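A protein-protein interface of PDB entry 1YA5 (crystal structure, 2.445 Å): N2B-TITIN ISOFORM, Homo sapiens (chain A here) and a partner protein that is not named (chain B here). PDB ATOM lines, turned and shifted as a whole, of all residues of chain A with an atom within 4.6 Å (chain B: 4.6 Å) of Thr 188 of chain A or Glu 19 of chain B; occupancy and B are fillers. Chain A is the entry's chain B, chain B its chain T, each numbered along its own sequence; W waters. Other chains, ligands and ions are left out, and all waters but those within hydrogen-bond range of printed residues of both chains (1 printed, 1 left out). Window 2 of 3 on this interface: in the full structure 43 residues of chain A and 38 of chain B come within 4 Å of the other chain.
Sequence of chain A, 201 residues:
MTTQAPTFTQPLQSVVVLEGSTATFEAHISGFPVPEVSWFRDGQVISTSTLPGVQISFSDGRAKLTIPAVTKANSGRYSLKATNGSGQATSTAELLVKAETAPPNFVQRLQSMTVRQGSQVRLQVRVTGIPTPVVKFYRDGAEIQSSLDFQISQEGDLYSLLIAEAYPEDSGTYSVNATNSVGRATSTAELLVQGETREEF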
ATOM      1  N   LEU A 110      -3.762   7.504  12.192  1.00  0.00           N
ATOM      2  CA  LEU A 110      -5.161   7.113  12.242  1.00  0.00           C
ATOM      3  C   LEU A 110      -5.702   7.309  13.660  1.00  0.00           C
ATOM      4  O   LEU A 110      -5.009   7.024  14.639  1.00  0.00           O
ATOM      5  CB  LEU A 110      -5.298   5.633  11.868  1.00  0.00           C
ATOM      6  CG  LEU A 110      -6.034   5.197  10.605  1.00  0.00           C
ATOM      7  CD1 LEU A 110      -5.656   6.012   9.413  1.00  0.00           C
ATOM      8  CD2 LEU A 110      -5.794   3.701  10.325  1.00  0.00           C
ATOM      9  N   GLN A 111      -6.933   7.787  13.775  1.00  0.00           N
ATOM     10  CA  GLN A 111      -7.594   7.802  15.062  1.00  0.00           C
ATOM     11  C   GLN A 111      -8.975   7.154  14.936  1.00  0.00           C
ATOM     12  O   GLN A 111      -9.646   7.317  13.918  1.00  0.00           O
ATOM     13  CB  GLN A 111      -7.633   9.222  15.652  1.00  0.00           C
ATOM     14  CG  GLN A 111      -6.260   9.913  15.692  1.00  0.00           C
ATOM     15  CD  GLN A 111      -5.429   9.596  16.939  1.00  0.00           C
ATOM     16  OE1 GLN A 111      -5.681  10.130  18.017  1.00  0.00           O
ATOM     17  NE2 GLN A 111      -4.415   8.745  16.838  1.00  0.00           N
ATOM     18  N   SER A 112      -9.392   6.393  15.937  1.00  0.00           N
ATOM     19  CA  SER A 112     -10.681   5.720  15.824  1.00  0.00           C
ATOM     20  C   SER A 112     -11.823   6.699  16.001  1.00  0.00           C
ATOM     21  O   SER A 112     -11.646   7.796  16.538  1.00  0.00           O
ATOM     22  CB  SER A 112     -10.796   4.532  16.788  1.00  0.00           C
ATOM     23  OG  SER A 112     -10.115   4.755  18.003  1.00  0.00           O
ATOM     24  N   THR A 173     -11.544  -2.660  12.170  1.00  0.00           N
ATOM     25  CA  THR A 173     -10.253  -2.113  12.491  1.00  0.00           C
ATOM     26  C   THR A 173      -9.563  -1.760  11.199  1.00  0.00           C
ATOM     27  O   THR A 173      -9.326  -2.608  10.343  1.00  0.00           O
ATOM     28  CB  THR A 173      -9.437  -3.075  13.360  1.00  0.00           C
ATOM     29  OG1 THR A 173     -10.231  -3.446  14.491  1.00  0.00           O
ATOM     30  CG2 THR A 173      -8.201  -2.384  13.916  1.00  0.00           C
ATOM     31  N   TYR A 174      -9.303  -0.474  11.039  1.00  0.00           N
ATOM     32  CA  TYR A 174      -8.562  -0.008   9.910  1.00  0.00           C
ATOM     33  C   TYR A 174      -7.123   0.148  10.321  1.00  0.00           C
ATOM     34  O   TYR A 174      -6.801   0.359  11.498  1.00  0.00           O
ATOM     35  CB  TYR A 174      -9.185   1.260   9.344  1.00  0.00           C
ATOM     36  CG  TYR A 174     -10.520   0.947   8.702  1.00  0.00           C
ATOM     37  CD1 TYR A 174     -11.670   0.809   9.474  1.00  0.00           C
ATOM     38  CD2 TYR A 174     -10.625   0.730   7.330  1.00  0.00           C
ATOM     39  CE1 TYR A 174     -12.866   0.491   8.903  1.00  0.00           C
ATOM     40  CE2 TYR A 174     -11.834   0.417   6.751  1.00  0.00           C
ATOM     41  CZ  TYR A 174     -12.943   0.291   7.540  1.00  0.00           C
ATOM     42  OH  TYR A 174     -14.152  -0.003   6.971  1.00  0.00           O
ATOM     43  N   SER A 175      -6.255  -0.039   9.346  1.00  0.00           N
ATOM     44  CA  SER A 175      -4.833   0.049   9.560  1.00  0.00           C
ATOM     45  C   SER A 175      -4.252   0.597   8.277  1.00  0.00           C
ATOM     46  O   SER A 175      -4.726   0.267   7.190  1.00  0.00           O
ATOM     47  CB  SER A 175      -4.255  -1.318   9.908  1.00  0.00           C
ATOM     48  OG  SER A 175      -4.080  -2.097   8.743  1.00  0.00           O
ATOM     49  N   THR A 186       3.262   1.294  11.164  1.00  0.00           N
ATOM     50  CA  THR A 186       1.861   0.911  11.057  1.00  0.00           C
ATOM     51  C   THR A 186       0.952   1.575  12.081  1.00  0.00           C
ATOM     52  O   THR A 186       1.233   1.568  13.275  1.00  0.00           O
ATOM     53  CB  THR A 186       1.695  -0.617  11.107  1.00  0.00           C
ATOM     54  OG1 THR A 186       2.492  -1.221  10.072  1.00  0.00           O
ATOM     55  CG2 THR A 186       0.240  -0.981  10.852  1.00  0.00           C
ATOM     56  N   SER A 187      -0.146   2.142  11.594  1.00  0.00           N
ATOM     57  CA  SER A 187      -1.120   2.856  12.428  1.00  0.00           C
ATOM     58  C   SER A 187      -2.485   2.183  12.332  1.00  0.00           C
ATOM     59  O   SER A 187      -3.008   2.006  11.250  1.00  0.00           O
ATOM     60  CB  SER A 187      -1.279   4.299  11.928  1.00  0.00           C
ATOM     61  OG  SER A 187      -2.055   5.077  12.828  1.00  0.00           O
ATOM     62  N   THR A 188      -3.074   1.825  13.457  1.00  0.00           N
ATOM     63  CA  THR A 188      -4.393   1.223  13.410  1.00  0.00           C
ATOM     64  C   THR A 188      -5.395   1.981  14.262  1.00  0.00           C
ATOM     65  O   THR A 188      -5.047   2.516  15.332  1.00  0.00           O
ATOM     66  CB  THR A 188      -4.361  -0.295  13.729  1.00  0.00           C
ATOM     67  OG1 THR A 188      -4.325  -0.496  15.130  1.00  0.00           O
ATOM     68  CG2 THR A 188      -3.102  -0.904  13.209  1.00  0.00           C
ATOM     69  N   ALA A 189      -6.628   2.033  13.751  1.00  0.00           N
ATOM     70  CA  ALA A 189      -7.792   2.578  14.447  1.00  0.00           C
ATOM     71  C   ALA A 189      -9.024   1.695  14.229  1.00  0.00           C
ATOM     72  O   ALA A 189      -9.090   0.946  13.248  1.00  0.00           O
ATOM     73  CB  ALA A 189      -8.081   3.958  13.951  1.00  0.00           C
ATOM     74  N   GLU B  12       3.225   0.579  20.350  1.00  0.00           N
ATOM     75  CA  GLU B  12       2.361   1.337  21.240  1.00  0.00           C
ATOM     76  C   GLU B  12       0.982   0.736  21.222  1.00  0.00           C
ATOM     77  O   GLU B  12       0.452   0.448  20.163  1.00  0.00           O
ATOM     78  CB  GLU B  12       2.272   2.803  20.796  1.00  0.00           C
ATOM     79  CG  GLU B  12       3.565   3.568  20.738  1.00  0.00           C
ATOM     80  CD  GLU B  12       3.349   5.099  20.816  1.00  0.00           C
ATOM     81  OE1 GLU B  12       4.329   5.842  20.996  1.00  0.00           O
ATOM     82  OE2 GLU B  12       2.209   5.570  20.706  1.00  0.00           O
ATOM     83  N   GLU B  13       0.388   0.549  22.393  1.00  0.00           N
ATOM     84  CA  GLU B  13      -1.013   0.114  22.456  1.00  0.00           C
ATOM     85  C   GLU B  13      -1.888   1.063  23.269  1.00  0.00           C
ATOM     86  O   GLU B  13      -1.742   1.228  24.477  1.00  0.00           O
ATOM     87  CB  GLU B  13      -1.156  -1.357  22.902  1.00  0.00           C
ATOM     88  CG  GLU B  13      -0.904  -1.623  24.392  1.00  0.00           C
ATOM     89  CD  GLU B  13      -2.141  -1.365  25.250  1.00  0.00           C
ATOM     90  OE1 GLU B  13      -3.239  -1.299  24.652  1.00  0.00           O
ATOM     91  OE2 GLU B  13      -2.041  -1.223  26.506  1.00  0.00           O
ATOM     92  N   ASN B  14      -2.807   1.696  22.577  1.00  0.00           N
ATOM     93  CA  ASN B  14      -3.867   2.430  23.220  1.00  0.00           C
ATOM     94  C   ASN B  14      -5.168   1.664  23.502  1.00  0.00           C
ATOM     95  O   ASN B  14      -5.925   1.376  22.584  1.00  0.00           O
ATOM     96  CB  ASN B  14      -4.230   3.595  22.357  1.00  0.00           C
ATOM     97  CG  ASN B  14      -4.929   4.613  23.133  1.00  0.00           C
ATOM     98  OD1 ASN B  14      -5.740   4.276  23.991  1.00  0.00           O
ATOM     99  ND2 ASN B  14      -4.603   5.858  22.900  1.00  0.00           N
ATOM    100  N   ARG B  17      -8.569   4.283  23.416  1.00  0.00           N
ATOM    101  CA  ARG B  17      -9.109   4.560  22.108  1.00  0.00           C
ATOM    102  C   ARG B  17      -8.891   3.409  21.122  1.00  0.00           C
ATOM    103  O   ARG B  17      -9.113   3.565  19.936  1.00  0.00           O
ATOM    104  CB  ARG B  17      -8.574   5.877  21.570  1.00  0.00           C
ATOM    105  CG  ARG B  17      -8.184   6.864  22.687  1.00  0.00           C
ATOM    106  CD  ARG B  17      -8.976   8.181  22.626  1.00  0.00           C
ATOM    107  NE  ARG B  17     -10.426   7.980  22.784  1.00  0.00           N
ATOM    108  CZ  ARG B  17     -11.290   7.969  21.765  1.00  0.00           C
ATOM    109  NH1 ARG B  17     -10.853   8.162  20.523  1.00  0.00           N
ATOM    110  NH2 ARG B  17     -12.588   7.769  21.977  1.00  0.00           N
ATOM    111  N   ARG B  18      -8.490   2.249  21.602  1.00  0.00           N
ATOM    112  CA  ARG B  18      -8.407   1.056  20.714  1.00  0.00           C
ATOM    113  C   ARG B  18      -7.593   1.335  19.472  1.00  0.00           C
ATOM    114  O   ARG B  18      -8.081   1.199  18.341  1.00  0.00           O
ATOM    115  CB  ARG B  18      -9.783   0.628  20.245  1.00  0.00           C
ATOM    116  CG  ARG B  18     -10.843   0.896  21.271  1.00  0.00           C
ATOM    117  CD  ARG B  18     -11.145  -0.379  21.994  1.00  0.00           C
ATOM    118  NE  ARG B  18     -10.576  -0.441  23.325  1.00  0.00           N
ATOM    119  CZ  ARG B  18     -10.167  -1.578  23.873  1.00  0.00           C
ATOM    120  NH1 ARG B  18     -10.255  -2.721  23.188  1.00  0.00           N
ATOM    121  NH2 ARG B  18      -9.670  -1.571  25.102  1.00  0.00           N
ATOM    122  N   GLU B  19      -6.349   1.746  19.704  1.00  0.00           N
ATOM    123  CA  GLU B  19      -5.412   2.090  18.653  1.00  0.00           C
ATOM    124  C   GLU B  19      -4.060   1.468  18.928  1.00  0.00           C
ATOM    125  O   GLU B  19      -3.669   1.268  20.070  1.00  0.00           O
ATOM    126  CB  GLU B  19      -5.240   3.589  18.565  1.00  0.00           C
ATOM    127  CG  GLU B  19      -6.413   4.312  17.967  1.00  0.00           C
ATOM    128  CD  GLU B  19      -6.431   5.775  18.430  1.00  0.00           C
ATOM    129  OE1 GLU B  19      -5.452   6.154  19.067  1.00  0.00           O
ATOM    130  OE2 GLU B  19      -7.392   6.509  18.159  1.00  0.00           O
ATOM    131  N   ALA B  20      -3.349   1.143  17.859  1.00  0.00           N
ATOM    132  CA  ALA B  20      -2.103   0.436  17.984  1.00  0.00           C
ATOM    133  C   ALA B  20      -1.189   1.006  16.922  1.00  0.00           C
ATOM    134  O   ALA B  20      -1.633   1.539  15.909  1.00  0.00           O
ATOM    135  CB  ALA B  20      -2.311  -1.073  17.757  1.00  0.00           C
ATOM    136  N   PHE B  21       0.101   0.874  17.142  1.00  0.00           N
ATOM    137  CA  PHE B  21       1.042   1.575  16.319  1.00  0.00           C
ATOM    138  C   PHE B  21       2.365   0.911  16.541  1.00  0.00           C
ATOM    139  O   PHE B  21       2.779   0.686  17.676  1.00  0.00           O
ATOM    140  CB  PHE B  21       1.177   3.046  16.758  1.00  0.00           C
ATOM    141  CG  PHE B  21       2.297   3.732  16.083  1.00  0.00           C
ATOM    142  CD1 PHE B  21       2.099   4.366  14.856  1.00  0.00           C
ATOM    143  CD2 PHE B  21       3.591   3.671  16.607  1.00  0.00           C
ATOM    144  CE1 PHE B  21       3.165   4.990  14.174  1.00  0.00           C
ATOM    145  CE2 PHE B  21       4.664   4.303  15.938  1.00  0.00           C
ATOM    146  CZ  PHE B  21       4.441   4.956  14.718  1.00  0.00           C
ATOM    147  N   TRP B  22       3.052   0.607  15.465  1.00  0.00           N
ATOM    148  CA  TRP B  22       4.386   0.153  15.627  1.00  0.00           C
ATOM    149  C   TRP B  22       5.297   0.596  14.501  1.00  0.00           C
ATOM    150  O   TRP B  22       4.834   1.077  13.471  1.00  0.00           O
ATOM    151  CB  TRP B  22       4.386  -1.337  15.870  1.00  0.00           C
ATOM    152  CG  TRP B  22       3.668  -2.202  14.909  1.00  0.00           C
ATOM    153  CD1 TRP B  22       4.237  -3.089  14.012  1.00  0.00           C
ATOM    154  CD2 TRP B  22       2.242  -2.402  14.812  1.00  0.00           C
ATOM    155  NE1 TRP B  22       3.251  -3.798  13.342  1.00  0.00           N
ATOM    156  CE2 TRP B  22       2.021  -3.404  13.809  1.00  0.00           C
ATOM    157  CE3 TRP B  22       1.125  -1.843  15.465  1.00  0.00           C
ATOM    158  CZ2 TRP B  22       0.722  -3.832  13.445  1.00  0.00           C
ATOM    159  CZ3 TRP B  22      -0.154  -2.267  15.096  1.00  0.00           C
ATOM    160  CH2 TRP B  22      -0.343  -3.254  14.093  1.00  0.00           C
HETATM  161  O   HOH W   1      -5.736   8.631  19.975  1.00  0.00           O
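The backbone carbonyl oxygen of Arg 17 of chain B is in hydrogen-bond range of the side-chain hydroxyl of Ser 112 of chain A, 2.5 Å away.
N of Ser 112 of chain A is in hydrogen-bond range of OE2 of Glu 19 of chain B, 3.0 Å away.
The backbone NH (N) of Thr 186 of chain A is in hydrogen-bond range of the backbone carbonyl oxygen (O) of Trp 22 of chain B.
O of Ala 20 of chain B lies within hydrogen-bond range of N of Thr 188 of chain A (2.9 Å).
N of Leu 110 of chain A lies within hydrogen-bond range of OG of Ser 187 of chain A (3.0 Å).
O of Phe 21 of chain B sits at hydrogen-bond distance from N of Glu 12 of chain B (2.7 Å).
N of Arg 17 of chain B sits at hydrogen-bond distance from OD1 of Asn 14 of chain B, 2.9 Å away.
O of Glu 19 of chain B is in hydrogen-bond range of N of Asn 14 of chain B (2.7 Å).
CA of Gln 111 of chain A touches OE2 of Glu 19 of chain B, at 3.4 Å.
Ala 20 of chain B touches Thr 186 of chain A (O to O, 3.9 Å).
Phe 21 of chain B touches Thr 186 of chain A (CA to O, 3.0 Å).
Ser 187 of chain A touches Ala 20 of chain B (C to O, 3.7 Å).
CA of Glu 19 of chain B touches O of Thr 188 of chain A, 3.4 Å away.
Trp 22 of chain B touches Thr 188 of chain A.
Printed residues of chain B within 4 Å of Ser 112 of chain A: Arg 17 and Glu 19.
Of the printed residues of chain B, Thr 186 of chain A touches Ala 20 (3.9 Å), Phe 21 (3.0 Å) and Trp 22 (2.8 Å).
Of chain B, only Glu 19 (3.4 Å), Ala 20 (2.9 Å) and Trp 22 (3.7 Å) come within 4 Å of Thr 188 of chain A.
Ala 189 of chain A touches none of the printed residues of chain B.
Arg 18 of chain B touches none of the printed residues of chain A.
Of chain A, only Gln 111, Ser 112 and Thr 188 come within 4 Å of Glu 19 of chain B.
The nearest residue of chain B that does not touch Thr 188 of chain A is Arg 18 of chain B (4.5 Å).
Among the printed residues, 10 pairs touch across the chains.
Among the printed residues, no Asp or Glu carboxylate lies within 4 Å of a Lys or Arg side-chain nitrogen of the other chain.
Water W1 lies within hydrogen-bond range of OE1 of Gln 111 of chain A (2.5 Å) and OE1 of Glu 19 of chain B (2.7 Å).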
